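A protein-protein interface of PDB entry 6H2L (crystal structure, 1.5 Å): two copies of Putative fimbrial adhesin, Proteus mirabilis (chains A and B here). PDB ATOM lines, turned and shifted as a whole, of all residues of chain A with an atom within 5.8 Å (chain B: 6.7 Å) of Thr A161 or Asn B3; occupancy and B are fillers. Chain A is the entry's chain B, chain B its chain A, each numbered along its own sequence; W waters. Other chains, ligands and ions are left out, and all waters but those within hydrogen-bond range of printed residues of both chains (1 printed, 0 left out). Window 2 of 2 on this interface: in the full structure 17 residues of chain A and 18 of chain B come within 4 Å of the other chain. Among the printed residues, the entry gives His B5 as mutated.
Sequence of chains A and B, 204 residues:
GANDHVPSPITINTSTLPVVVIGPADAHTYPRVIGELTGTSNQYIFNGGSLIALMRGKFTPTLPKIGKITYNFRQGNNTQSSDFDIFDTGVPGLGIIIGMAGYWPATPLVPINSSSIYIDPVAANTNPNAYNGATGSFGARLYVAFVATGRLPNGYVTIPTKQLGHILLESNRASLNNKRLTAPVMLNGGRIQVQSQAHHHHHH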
ATOM      1  N   ILE A 159       9.797  -8.540  19.846  1.00  0.00           N
ATOM      2  CA  ILE A 159       9.703  -9.752  20.656  1.00  0.00           C
ATOM      3  C   ILE A 159      11.107 -10.339  20.761  1.00  0.00           C
ATOM      4  O   ILE A 159      11.684 -10.708  19.729  1.00  0.00           O
ATOM      5  CB  ILE A 159       8.728 -10.764  20.032  1.00  0.00           C
ATOM      6  CG1 ILE A 159       7.365 -10.112  19.750  1.00  0.00           C
ATOM      7  CG2 ILE A 159       8.573 -11.970  20.943  1.00  0.00           C
ATOM      8  CD1 ILE A 159       6.726  -9.481  20.943  1.00  0.00           C
ATOM      9  N   PRO A 160      11.691 -10.434  21.945  1.00  0.00           N
ATOM     10  CA  PRO A 160      13.027 -11.029  22.050  1.00  0.00           C
ATOM     11  C   PRO A 160      12.965 -12.529  21.850  1.00  0.00           C
ATOM     12  O   PRO A 160      11.948 -13.165  22.126  1.00  0.00           O
ATOM     13  CB  PRO A 160      13.471 -10.675  23.476  1.00  0.00           C
ATOM     14  CG  PRO A 160      12.529  -9.634  23.954  1.00  0.00           C
ATOM     15  CD  PRO A 160      11.228  -9.886  23.228  1.00  0.00           C
ATOM     16  N   THR A 161      14.075 -13.082  21.375  1.00  0.00           N
ATOM     17  CA  THR A 161      14.249 -14.534  21.389  1.00  0.00           C
ATOM     18  C   THR A 161      14.149 -15.039  22.826  1.00  0.00           C
ATOM     19  O   THR A 161      14.760 -14.474  23.741  1.00  0.00           O
ATOM     20  CB  THR A 161      15.581 -14.913  20.778  1.00  0.00           C
ATOM     21  OG1 THR A 161      15.583 -14.636  19.397  1.00  0.00           O
ATOM     22  CG2 THR A 161      15.857 -16.424  20.949  1.00  0.00           C
ATOM     23  N   LYS A 162      13.344 -16.080  23.036  1.00  0.00           N
ATOM     24  CA  LYS A 162      13.110 -16.636  24.360  1.00  0.00           C
ATOM     25  C   LYS A 162      13.236 -18.154  24.284  1.00  0.00           C
ATOM     26  O   LYS A 162      12.742 -18.789  23.343  1.00  0.00           O
ATOM     27  CB  LYS A 162      11.740 -16.262  24.895  1.00  0.00           C
ATOM     28  CG  LYS A 162      11.585 -14.770  25.211  1.00  0.00           C
ATOM     29  CD  LYS A 162      12.496 -14.358  26.354  1.00  0.00           C
ATOM     30  CE  LYS A 162      12.147 -12.975  26.882  1.00  0.00           C
ATOM     31  NZ  LYS A 162      13.167 -12.482  27.850  1.00  0.00           N
ATOM     32  N   GLN A 163      13.891 -18.730  25.288  1.00  0.00           N
ATOM     33  CA  GLN A 163      13.856 -20.175  25.480  1.00  0.00           C
ATOM     34  C   GLN A 163      12.540 -20.531  26.160  1.00  0.00           C
ATOM     35  O   GLN A 163      12.239 -20.008  27.244  1.00  0.00           O
ATOM     36  CB  GLN A 163      15.043 -20.624  26.330  1.00  0.00           C
ATOM     37  CG  GLN A 163      15.058 -22.130  26.560  1.00  0.00           C
ATOM     38  CD  GLN A 163      16.279 -22.599  27.313  1.00  0.00           C
ATOM     39  OE1 GLN A 163      16.183 -23.071  28.447  1.00  0.00           O
ATOM     40  NE2 GLN A 163      17.444 -22.453  26.693  1.00  0.00           N
ATOM     41  N   MET A 186      13.017 -23.228  21.474  1.00  0.00           N
ATOM     42  CA  MET A 186      13.277 -21.808  21.309  1.00  0.00           C
ATOM     43  C   MET A 186      12.159 -21.122  20.545  1.00  0.00           C
ATOM     44  O   MET A 186      11.626 -21.665  19.572  1.00  0.00           O
ATOM     45  CB  MET A 186      14.610 -21.596  20.557  1.00  0.00           C
ATOM     46  CG  MET A 186      15.842 -22.245  21.208  1.00  0.00           C
ATOM     47  SD  MET A 186      16.225 -21.560  22.844  1.00  0.00           S
ATOM     48  CE  MET A 186      16.534 -19.833  22.445  1.00  0.00           C
ATOM     49  N   LEU A 187      11.796 -19.920  21.015  1.00  0.00           N
ATOM     50  CA  LEU A 187      10.983 -18.980  20.252  1.00  0.00           C
ATOM     51  C   LEU A 187      11.920 -17.928  19.658  1.00  0.00           C
ATOM     52  O   LEU A 187      12.465 -17.092  20.405  1.00  0.00           O
ATOM     53  CB  LEU A 187       9.921 -18.332  21.136  1.00  0.00           C
ATOM     54  CG  LEU A 187       9.217 -17.095  20.528  1.00  0.00           C
ATOM     55  CD1 LEU A 187       8.464 -17.443  19.282  1.00  0.00           C
ATOM     56  CD2 LEU A 187       8.298 -16.406  21.554  1.00  0.00           C
ATOM     57  N   ASN A 188      12.140 -17.989  18.341  1.00  0.00           N
ATOM     58  CA  ASN A 188      12.971 -16.998  17.670  1.00  0.00           C
ATOM     59  C   ASN A 188      12.261 -15.654  17.722  1.00  0.00           C
ATOM     60  O   ASN A 188      11.075 -15.555  17.386  1.00  0.00           O
ATOM     61  CB  ASN A 188      13.240 -17.383  16.226  1.00  0.00           C
ATOM     62  CG  ASN A 188      14.447 -18.294  16.074  1.00  0.00           C
ATOM     63  OD1 ASN A 188      15.286 -18.400  16.976  1.00  0.00           O
ATOM     64  ND2 ASN A 188      14.548 -18.952  14.921  1.00  0.00           N
ATOM     65  N   GLY A 189      12.980 -14.634  18.143  1.00  0.00           N
ATOM     66  CA  GLY A 189      12.407 -13.313  18.272  1.00  0.00           C
ATOM     67  C   GLY A 189      12.168 -12.659  16.928  1.00  0.00           C
ATOM     68  O   GLY A 189      12.584 -13.125  15.859  1.00  0.00           O
ATOM     69  N   GLY A 190      11.522 -11.508  16.992  1.00  0.00           N
ATOM     70  CA  GLY A 190      11.215 -10.758  15.789  1.00  0.00           C
ATOM     71  C   GLY A 190      10.362  -9.567  16.165  1.00  0.00           C
ATOM     72  O   GLY A 190      10.101  -9.316  17.329  1.00  0.00           O
ATOM     73  N   GLY B   1      13.622  -7.319  26.914  1.00  0.00           N
ATOM     74  CA  GLY B   1      14.521  -6.556  26.069  1.00  0.00           C
ATOM     75  C   GLY B   1      15.690  -7.369  25.551  1.00  0.00           C
ATOM     76  O   GLY B   1      16.055  -7.264  24.378  1.00  0.00           O
ATOM     77  N   ALA B   2      16.273  -8.193  26.419  1.00  0.00           N
ATOM     78  CA  ALA B   2      17.427  -8.985  26.036  1.00  0.00           C
ATOM     79  C   ALA B   2      17.000 -10.287  25.366  1.00  0.00           C
ATOM     80  O   ALA B   2      16.035 -10.931  25.783  1.00  0.00           O
ATOM     81  CB  ALA B   2      18.296  -9.301  27.260  1.00  0.00           C
ATOM     82  N   ASN B   3      17.742 -10.674  24.337  1.00  0.00           N
ATOM     83  CA  ASN B   3      17.499 -11.924  23.641  1.00  0.00           C
ATOM     84  C   ASN B   3      18.147 -13.082  24.382  1.00  0.00           C
ATOM     85  O   ASN B   3      19.272 -12.969  24.867  1.00  0.00           O
ATOM     86  CB  ASN B   3      18.058 -11.858  22.217  1.00  0.00           C
ATOM     87  CG  ASN B   3      17.258 -10.973  21.309  1.00  0.00           C
ATOM     88  OD1 ASN B   3      16.035 -11.081  21.233  1.00  0.00           O
ATOM     89  ND2 ASN B   3      17.945 -10.066  20.615  1.00  0.00           N
ATOM     90  N   ASP B   4      17.431 -14.200  24.466  1.00  0.00           N
ATOM     91  CA  ASP B   4      18.052 -15.446  24.867  1.00  0.00           C
ATOM     92  C   ASP B   4      18.877 -15.994  23.703  1.00  0.00           C
ATOM     93  O   ASP B   4      18.650 -15.666  22.540  1.00  0.00           O
ATOM     94  CB  ASP B   4      17.001 -16.478  25.295  1.00  0.00           C
ATOM     95  CG  ASP B   4      16.313 -16.101  26.600  1.00  0.00           C
ATOM     96  OD1 ASP B   4      16.794 -15.171  27.295  1.00  0.00           O
ATOM     97  OD2 ASP B   4      15.273 -16.717  26.935  1.00  0.00           O
ATOM     98  N   HIS B   5      19.846 -16.831  24.036  1.00  0.00           N
ATOM     99  CA  HIS B   5      20.707 -17.488  23.060  1.00  0.00           C
ATOM    100  C   HIS B   5      20.833 -18.949  23.425  1.00  0.00           C
ATOM    101  O   HIS B   5      20.924 -19.284  24.609  1.00  0.00           O
ATOM    102  CB  HIS B   5      22.101 -16.837  23.009  1.00  0.00           C
ATOM    103  CG  HIS B   5      22.098 -15.468  22.405  1.00  0.00           C
ATOM    104  ND1 HIS B   5      22.395 -15.239  21.078  1.00  0.00           N
ATOM    105  CD2 HIS B   5      21.823 -14.258  22.943  1.00  0.00           C
ATOM    106  CE1 HIS B   5      22.314 -13.945  20.827  1.00  0.00           C
ATOM    107  NE2 HIS B   5      21.949 -13.328  21.937  1.00  0.00           N
ATOM    108  N   VAL B   6      20.817 -19.807  22.406  1.00  0.00           N
ATOM    109  CA  VAL B   6      21.052 -21.238  22.591  1.00  0.00           C
ATOM    110  C   VAL B   6      22.414 -21.411  23.263  1.00  0.00           C
ATOM    111  O   VAL B   6      23.432 -20.960  22.711  1.00  0.00           O
ATOM    112  CB  VAL B   6      21.004 -21.987  21.253  1.00  0.00           C
ATOM    113  CG1 VAL B   6      21.481 -23.421  21.427  1.00  0.00           C
ATOM    114  CG2 VAL B   6      19.610 -21.956  20.665  1.00  0.00           C
ATOM    115  N   ASN B  47      25.131 -16.668  26.571  1.00  0.00           N
ATOM    116  CA  ASN B  47      25.163 -15.316  26.005  1.00  0.00           C
ATOM    117  C   ASN B  47      23.864 -14.631  26.379  1.00  0.00           C
ATOM    118  O   ASN B  47      22.802 -14.999  25.865  1.00  0.00           O
ATOM    119  CB  ASN B  47      25.352 -15.363  24.490  1.00  0.00           C
ATOM    120  CG  ASN B  47      25.307 -13.996  23.852  1.00  0.00           C
ATOM    121  OD1 ASN B  47      25.160 -12.986  24.533  1.00  0.00           O
ATOM    122  ND2 ASN B  47      25.431 -13.957  22.528  1.00  0.00           N
ATOM    123  N   GLY B  48      23.949 -13.649  27.274  1.00  0.00           N
ATOM    124  CA  GLY B  48      22.785 -12.939  27.737  1.00  0.00           C
ATOM    125  C   GLY B  48      22.336 -11.805  26.851  1.00  0.00           C
ATOM    126  O   GLY B  48      21.419 -11.070  27.224  1.00  0.00           O
ATOM    127  N   GLY B  49      22.962 -11.627  25.691  1.00  0.00           N
ATOM    128  CA  GLY B  49      22.591 -10.522  24.821  1.00  0.00           C
ATOM    129  C   GLY B  49      22.904  -9.197  25.490  1.00  0.00           C
ATOM    130  O   GLY B  49      23.992  -8.996  26.042  1.00  0.00           O
ATOM    131  N   SER B  50      21.937  -8.280  25.445  1.00  0.00           N
ATOM    132  CA  SER B  50      22.084  -6.989  26.105  1.00  0.00           C
ATOM    133  C   SER B  50      21.935  -7.080  27.618  1.00  0.00           C
ATOM    134  O   SER B  50      22.089  -6.062  28.308  1.00  0.00           O
ATOM    135  CB  SER B  50      21.052  -5.997  25.558  1.00  0.00           C
ATOM    136  OG  SER B  50      19.737  -6.409  25.883  1.00  0.00           O
ATOM    137  N   LEU B  51      21.629  -8.261  28.149  1.00  0.00           N
ATOM    138  CA  LEU B  51      21.428  -8.412  29.580  1.00  0.00           C
ATOM    139  C   LEU B  51      22.762  -8.291  30.312  1.00  0.00           C
ATOM    140  O   LEU B  51      23.802  -8.744  29.830  1.00  0.00           O
ATOM    141  CB  LEU B  51      20.784  -9.766  29.872  1.00  0.00           C
ATOM    142  CG  LEU B  51      20.276 -10.036  31.289  1.00  0.00           C
ATOM    143  CD1 LEU B  51      19.024  -9.216  31.531  1.00  0.00           C
ATOM    144  CD2 LEU B  51      20.009 -11.518  31.502  1.00  0.00           C
HETATM  145  O   HOH W   1      14.171  -9.969  18.528  1.00  0.00           O
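N of Thr A161 sits at hydrogen-bond distance from OD1 of Asn B3, at 2.8 Å. The backbone NH of Asp B4 sits at hydrogen-bond distance from the backbone carbonyl oxygen of Thr A161 (2.8 Å). The side-chain carboxylate (OD2) of Asp B4 sits at hydrogen-bond distance from the backbone NH (N) of Gln A163 (2.9 Å).
The side-chain hydroxyl of Thr A161 sits at hydrogen-bond distance from the backbone NH of Gly A189, at 2.9 Å. The backbone carbonyl oxygen of Lys A162 lies within hydrogen-bond range of the backbone NH of Leu A187 (2.8 Å).
Among the printed residues, merely in contact across the chains: Pro A160 with Asn B3 (3.1 Å), Lys A162 with Asp B4 (3.4 Å), Pro A160 with Ala B2 (3.5 Å), Met A186 with Val B6 (3.8 Å), Lys A162 with Ala B2 (3.9 Å) and Pro A160 with Gly B1 (3.9 Å).
Thr A161 touches just these residues of chain B: Asn B3 (2.8 Å) and Asp B4 (2.8 Å). Of chain A, only Pro A160 (3.1 Å) and Thr A161 (2.8 Å) come within 4 Å of Asn B3. Printed residues of chain A within 4 Å of Asp B4: Thr A161, Lys A162 and Gln A163. Of the printed residues of chain B, Met A186 touches Val B6 (3.8 Å). The nearest residue of chain B that does not touch Thr A161 is Ala B2 (4.3 Å). The nearest printed residue of chain A that does not touch Gly B1 is Lys A162 (5.3 Å).
Hydrophobic or aromatic side chains of chain B that line the printed part of chain A: Val B6. Among the printed residues, 9 pairs touch across the chains. Among the printed residues, no Asp or Glu carboxylate lies within 4 Å of a Lys or Arg side-chain nitrogen of the other chain.
No position is printed for both chains. Of the 9 pairs that touch across the chains among the printed residues, none has its exchanged pair printed and touching as well.
Water W1 lies within hydrogen-bond range of the backbone carbonyl oxygen (O) of Ile A159 (2.9 Å), the backbone NH (N) of Gly A190 (3.4 Å) and the side-chain amide oxygen (OD1) of Asn B3 (3.5 Å).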
